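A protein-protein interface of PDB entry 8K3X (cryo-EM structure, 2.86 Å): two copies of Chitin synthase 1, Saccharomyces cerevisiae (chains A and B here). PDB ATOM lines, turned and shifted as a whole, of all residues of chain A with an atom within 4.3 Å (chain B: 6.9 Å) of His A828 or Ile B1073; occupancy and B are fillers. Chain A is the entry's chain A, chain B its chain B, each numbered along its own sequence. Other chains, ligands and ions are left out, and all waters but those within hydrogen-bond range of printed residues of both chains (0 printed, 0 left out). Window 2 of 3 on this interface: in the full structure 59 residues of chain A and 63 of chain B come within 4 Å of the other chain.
No position is printed for both chains.
Of the 5 pairs that touch across the chains among the printed residues, none has its exchanged pair printed and touching as well.
His A828 touches just these residues of chain B: Ile B1073 and Ser B1074.
Ile B1073 touches just one residue of chain A: His A828.
Printed residues of chain B within 4 Å of Ala A824: Met B1070.
Of the printed residues of chain B, Asn A832 touches Met B1070.
Printed residues of chain B within 4 Å of Leu A825: Met B1070 (3.7 Å).
Printed residues of chain A within 4 Å of Met B1070: Ala A824 (3.4 Å), Leu A825 (3.7 Å) and Asn A832 (3.4 Å).
Of the printed residues of chain A, Ser B1074 touches His A828 (3.7 Å).
The nearest residue of chain B that does not touch His A828 is Met B1070 (4.2 Å).
The nearest residue of chain A that does not touch Ile B1073 is Leu A825 (4.1 Å).
The nearest printed residue of chain B that does not touch Asn A832 is Lys B1071 (4.2 Å).
The backbone carbonyl oxygen (O) of His A828 is in hydrogen-bond range of the side-chain amide nitrogen (ND2) of Asn A832.
Among the printed residues, pairs that only touch across the chains: Ala A824 with Met B1070 (3.4 Å), Leu A825 with Met B1070 (3.7 Å), His A828 with Ile B1073 (3.6 Å), His A828 with Ser B1074 (3.7 Å) and Asn A832 with Met B1070 (3.4 Å).
Of the 9 printed residues of chain A, 4 touch a printed residue of chain B.
Hydrophobic or aromatic side chains of chain A that line the printed part of chain B: Ala A824, Leu A825 and His A828.
Of the 10 printed residues of chain B, 3 touch a printed residue of chain A.
Printed residues of chain B that touch a printed residue of chain A: Met B1070, Ile B1073 and Ser B1074.
Hydrophobic or aromatic side chains of chain B within 4 Å of the printed part of chain A: Met B1070 and Ile B1073.
Among the printed residues, 5 pairs touch across the chains.
Among the printed residues, no Asp or Glu carboxylate lies within 4 Å of a Lys or Arg side-chain nitrogen of the other chain.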
ATOM      1  N   ILE A 823      24.039  -3.678  -3.774  1.00  0.00           N
ATOM      2  CA  ILE A 823      25.289  -3.907  -3.055  1.00  0.00           C
ATOM      3  C   ILE A 823      26.414  -3.057  -3.640  1.00  0.00           C
ATOM      4  O   ILE A 823      27.243  -2.511  -2.905  1.00  0.00           O
ATOM      5  CB  ILE A 823      25.649  -5.402  -3.028  1.00  0.00           C
ATOM      6  CG1 ILE A 823      26.766  -5.652  -2.025  1.00  0.00           C
ATOM      7  CG2 ILE A 823      26.079  -5.893  -4.372  1.00  0.00           C
ATOM      8  CD1 ILE A 823      27.030  -7.098  -1.770  1.00  0.00           C
ATOM      9  N   ALA A 824      26.446  -2.902  -4.963  1.00  0.00           N
ATOM     10  CA  ALA A 824      27.488  -2.098  -5.587  1.00  0.00           C
ATOM     11  C   ALA A 824      27.351  -0.636  -5.222  1.00  0.00           C
ATOM     12  O   ALA A 824      28.346   0.030  -4.937  1.00  0.00           O
ATOM     13  CB  ALA A 824      27.445  -2.264  -7.097  1.00  0.00           C
ATOM     14  N   LEU A 825      26.126  -0.114  -5.240  1.00  0.00           N
ATOM     15  CA  LEU A 825      25.897   1.255  -4.791  1.00  0.00           C
ATOM     16  C   LEU A 825      26.291   1.435  -3.338  1.00  0.00           C
ATOM     17  O   LEU A 825      26.657   2.538  -2.924  1.00  0.00           O
ATOM     18  CB  LEU A 825      24.432   1.632  -4.963  1.00  0.00           C
ATOM     19  CG  LEU A 825      23.966   1.970  -6.361  1.00  0.00           C
ATOM     20  CD1 LEU A 825      22.511   2.323  -6.314  1.00  0.00           C
ATOM     21  CD2 LEU A 825      24.772   3.128  -6.855  1.00  0.00           C
ATOM     22  N   ALA A 826      26.194   0.375  -2.544  1.00  0.00           N
ATOM     23  CA  ALA A 826      26.547   0.493  -1.140  1.00  0.00           C
ATOM     24  C   ALA A 826      28.054   0.474  -0.921  1.00  0.00           C
ATOM     25  O   ALA A 826      28.560   1.227  -0.083  1.00  0.00           O
ATOM     26  CB  ALA A 826      25.881  -0.621  -0.341  1.00  0.00           C
ATOM     27  N   TYR A 827      28.800  -0.355  -1.655  1.00  0.00           N
ATOM     28  CA  TYR A 827      30.196  -0.580  -1.288  1.00  0.00           C
ATOM     29  C   TYR A 827      31.229  -0.413  -2.393  1.00  0.00           C
ATOM     30  O   TYR A 827      32.421  -0.366  -2.073  1.00  0.00           O
ATOM     31  CB  TYR A 827      30.342  -1.962  -0.655  1.00  0.00           C
ATOM     32  CG  TYR A 827      29.484  -2.030   0.566  1.00  0.00           C
ATOM     33  CD1 TYR A 827      28.416  -2.897   0.644  1.00  0.00           C
ATOM     34  CD2 TYR A 827      29.712  -1.171   1.626  1.00  0.00           C
ATOM     35  CE1 TYR A 827      27.618  -2.928   1.764  1.00  0.00           C
ATOM     36  CE2 TYR A 827      28.924  -1.194   2.743  1.00  0.00           C
ATOM     37  CZ  TYR A 827      27.878  -2.074   2.809  1.00  0.00           C
ATOM     38  OH  TYR A 827      27.085  -2.097   3.925  1.00  0.00           O
ATOM     39  N   HIS A 828      30.842  -0.355  -3.661  1.00  0.00           N
ATOM     40  CA  HIS A 828      31.695   0.182  -4.717  1.00  0.00           C
ATOM     41  C   HIS A 828      32.896  -0.676  -5.086  1.00  0.00           C
ATOM     42  O   HIS A 828      33.565  -0.385  -6.080  1.00  0.00           O
ATOM     43  CB  HIS A 828      32.251   1.558  -4.337  1.00  0.00           C
ATOM     44  CG  HIS A 828      31.251   2.484  -3.732  1.00  0.00           C
ATOM     45  ND1 HIS A 828      30.356   3.208  -4.488  1.00  0.00           N
ATOM     46  CD2 HIS A 828      31.024   2.830  -2.445  1.00  0.00           C
ATOM     47  CE1 HIS A 828      29.608   3.946  -3.690  1.00  0.00           C
ATOM     48  NE2 HIS A 828      29.994   3.736  -2.444  1.00  0.00           N
ATOM     49  N   SER A 829      33.199  -1.718  -4.327  1.00  0.00           N
ATOM     50  CA  SER A 829      34.560  -2.226  -4.416  1.00  0.00           C
ATOM     51  C   SER A 829      34.819  -2.947  -5.724  1.00  0.00           C
ATOM     52  O   SER A 829      35.527  -2.440  -6.592  1.00  0.00           O
ATOM     53  CB  SER A 829      34.848  -3.162  -3.249  1.00  0.00           C
ATOM     54  OG  SER A 829      36.155  -3.688  -3.343  1.00  0.00           O
ATOM     55  N   ALA A 830      34.211  -4.102  -5.886  1.00  0.00           N
ATOM     56  CA  ALA A 830      34.323  -4.862  -7.120  1.00  0.00           C
ATOM     57  C   ALA A 830      32.957  -5.369  -7.536  1.00  0.00           C
ATOM     58  O   ALA A 830      32.873  -6.266  -8.376  1.00  0.00           O
ATOM     59  CB  ALA A 830      35.288  -6.032  -6.968  1.00  0.00           C
ATOM     60  N   ASN A 832      30.660  -3.473  -8.963  1.00  0.00           N
ATOM     61  CA  ASN A 832      30.280  -2.876 -10.236  1.00  0.00           C
ATOM     62  C   ASN A 832      30.493  -3.865 -11.372  1.00  0.00           C
ATOM     63  O   ASN A 832      29.578  -4.155 -12.162  1.00  0.00           O
ATOM     64  CB  ASN A 832      31.109  -1.623 -10.494  1.00  0.00           C
ATOM     65  CG  ASN A 832      31.166  -0.712  -9.314  1.00  0.00           C
ATOM     66  OD1 ASN A 832      30.187  -0.529  -8.613  1.00  0.00           O
ATOM     67  ND2 ASN A 832      32.321  -0.117  -9.089  1.00  0.00           N
ATOM     68  N   ILE B1068      29.264   2.860 -15.134  1.00  0.00           N
ATOM     69  CA  ILE B1068      30.034   4.096 -15.151  1.00  0.00           C
ATOM     70  C   ILE B1068      29.597   5.013 -14.020  1.00  0.00           C
ATOM     71  O   ILE B1068      30.426   5.658 -13.368  1.00  0.00           O
ATOM     72  CB  ILE B1068      29.900   4.778 -16.519  1.00  0.00           C
ATOM     73  CG1 ILE B1068      30.550   3.916 -17.589  1.00  0.00           C
ATOM     74  CG2 ILE B1068      30.536   6.136 -16.489  1.00  0.00           C
ATOM     75  CD1 ILE B1068      30.240   4.359 -18.969  1.00  0.00           C
ATOM     76  N   ALA B1069      28.291   5.091 -13.770  1.00  0.00           N
ATOM     77  CA  ALA B1069      27.813   5.937 -12.684  1.00  0.00           C
ATOM     78  C   ALA B1069      28.338   5.455 -11.341  1.00  0.00           C
ATOM     79  O   ALA B1069      28.763   6.261 -10.504  1.00  0.00           O
ATOM     80  CB  ALA B1069      26.289   5.972 -12.679  1.00  0.00           C
ATOM     81  N   MET B1070      28.317   4.145 -11.115  1.00  0.00           N
ATOM     82  CA  MET B1070      28.785   3.632  -9.836  1.00  0.00           C
ATOM     83  C   MET B1070      30.282   3.856  -9.680  1.00  0.00           C
ATOM     84  O   MET B1070      30.754   4.153  -8.578  1.00  0.00           O
ATOM     85  CB  MET B1070      28.430   2.155  -9.682  1.00  0.00           C
ATOM     86  CG  MET B1070      26.939   1.885  -9.587  1.00  0.00           C
ATOM     87  SD  MET B1070      26.495   0.157  -9.326  1.00  0.00           S
ATOM     88  CE  MET B1070      26.797  -0.585 -10.914  1.00  0.00           C
ATOM     89  N   LYS B1071      31.044   3.737 -10.770  1.00  0.00           N
ATOM     90  CA  LYS B1071      32.464   4.077 -10.703  1.00  0.00           C
ATOM     91  C   LYS B1071      32.664   5.532 -10.312  1.00  0.00           C
ATOM     92  O   LYS B1071      33.512   5.847  -9.473  1.00  0.00           O
ATOM     93  CB  LYS B1071      33.142   3.804 -12.041  1.00  0.00           C
ATOM     94  CG  LYS B1071      33.746   2.435 -12.169  1.00  0.00           C
ATOM     95  CD  LYS B1071      34.233   2.215 -13.579  1.00  0.00           C
ATOM     96  CE  LYS B1071      35.282   3.235 -13.949  1.00  0.00           C
ATOM     97  NZ  LYS B1071      35.795   3.010 -15.323  1.00  0.00           N
ATOM     98  N   SER B1072      31.889   6.436 -10.914  1.00  0.00           N
ATOM     99  CA  SER B1072      32.008   7.850 -10.576  1.00  0.00           C
ATOM    100  C   SER B1072      31.701   8.093  -9.107  1.00  0.00           C
ATOM    101  O   SER B1072      32.340   8.929  -8.462  1.00  0.00           O
ATOM    102  CB  SER B1072      31.076   8.680 -11.454  1.00  0.00           C
ATOM    103  OG  SER B1072      29.722   8.420 -11.130  1.00  0.00           O
ATOM    104  N   ILE B1073      30.708   7.383  -8.567  1.00  0.00           N
ATOM    105  CA  ILE B1073      30.416   7.513  -7.140  1.00  0.00           C
ATOM    106  C   ILE B1073      31.558   6.966  -6.296  1.00  0.00           C
ATOM    107  O   ILE B1073      31.843   7.491  -5.212  1.00  0.00           O
ATOM    108  CB  ILE B1073      29.092   6.821  -6.774  1.00  0.00           C
ATOM    109  CG1 ILE B1073      27.939   7.367  -7.607  1.00  0.00           C
ATOM    110  CG2 ILE B1073      28.782   7.012  -5.306  1.00  0.00           C
ATOM    111  CD1 ILE B1073      26.631   6.700  -7.299  1.00  0.00           C
ATOM    112  N   SER B1074      32.225   5.906  -6.764  1.00  0.00           N
ATOM    113  CA  SER B1074      33.229   5.236  -5.942  1.00  0.00           C
ATOM    114  C   SER B1074      34.379   6.159  -5.567  1.00  0.00           C
ATOM    115  O   SER B1074      34.990   5.986  -4.505  1.00  0.00           O
ATOM    116  CB  SER B1074      33.767   4.004  -6.666  1.00  0.00           C
ATOM    117  OG  SER B1074      34.927   3.505  -6.024  1.00  0.00           O
ATOM    118  N   THR B1075      34.694   7.134  -6.413  1.00  0.00           N
ATOM    119  CA  THR B1075      35.785   8.063  -6.141  1.00  0.00           C
ATOM    120  C   THR B1075      35.460   8.976  -4.963  1.00  0.00           C
ATOM    121  O   THR B1075      34.298   9.144  -4.594  1.00  0.00           O
ATOM    122  CB  THR B1075      36.104   8.926  -7.369  1.00  0.00           C
ATOM    123  OG1 THR B1075      35.054   9.880  -7.571  1.00  0.00           O
ATOM    124  CG2 THR B1075      36.233   8.054  -8.605  1.00  0.00           C
ATOM    125  N   ALA B1085      25.776   9.912  -7.958  1.00  0.00           N
ATOM    126  CA  ALA B1085      25.854  10.439  -9.314  1.00  0.00           C
ATOM    127  C   ALA B1085      24.686   9.944 -10.154  1.00  0.00           C
ATOM    128  O   ALA B1085      23.911   9.093  -9.722  1.00  0.00           O
ATOM    129  CB  ALA B1085      27.172  10.059  -9.959  1.00  0.00           C
ATOM    130  N   GLU B1086      24.576  10.473 -11.367  1.00  0.00           N
ATOM    131  CA  GLU B1086      23.392  10.288 -12.182  1.00  0.00           C
ATOM    132  C   GLU B1086      23.787   9.916 -13.603  1.00  0.00           C
ATOM    133  O   GLU B1086      24.880  10.243 -14.070  1.00  0.00           O
ATOM    134  CB  GLU B1086      22.540  11.556 -12.193  1.00  0.00           C
ATOM    135  CG  GLU B1086      22.122  12.040 -10.814  1.00  0.00           C
ATOM    136  CD  GLU B1086      21.223  11.058 -10.095  1.00  0.00           C
ATOM    137  OE1 GLU B1086      20.150  10.730 -10.639  1.00  0.00           O
ATOM    138  OE2 GLU B1086      21.593  10.607  -8.992  1.00  0.00           O
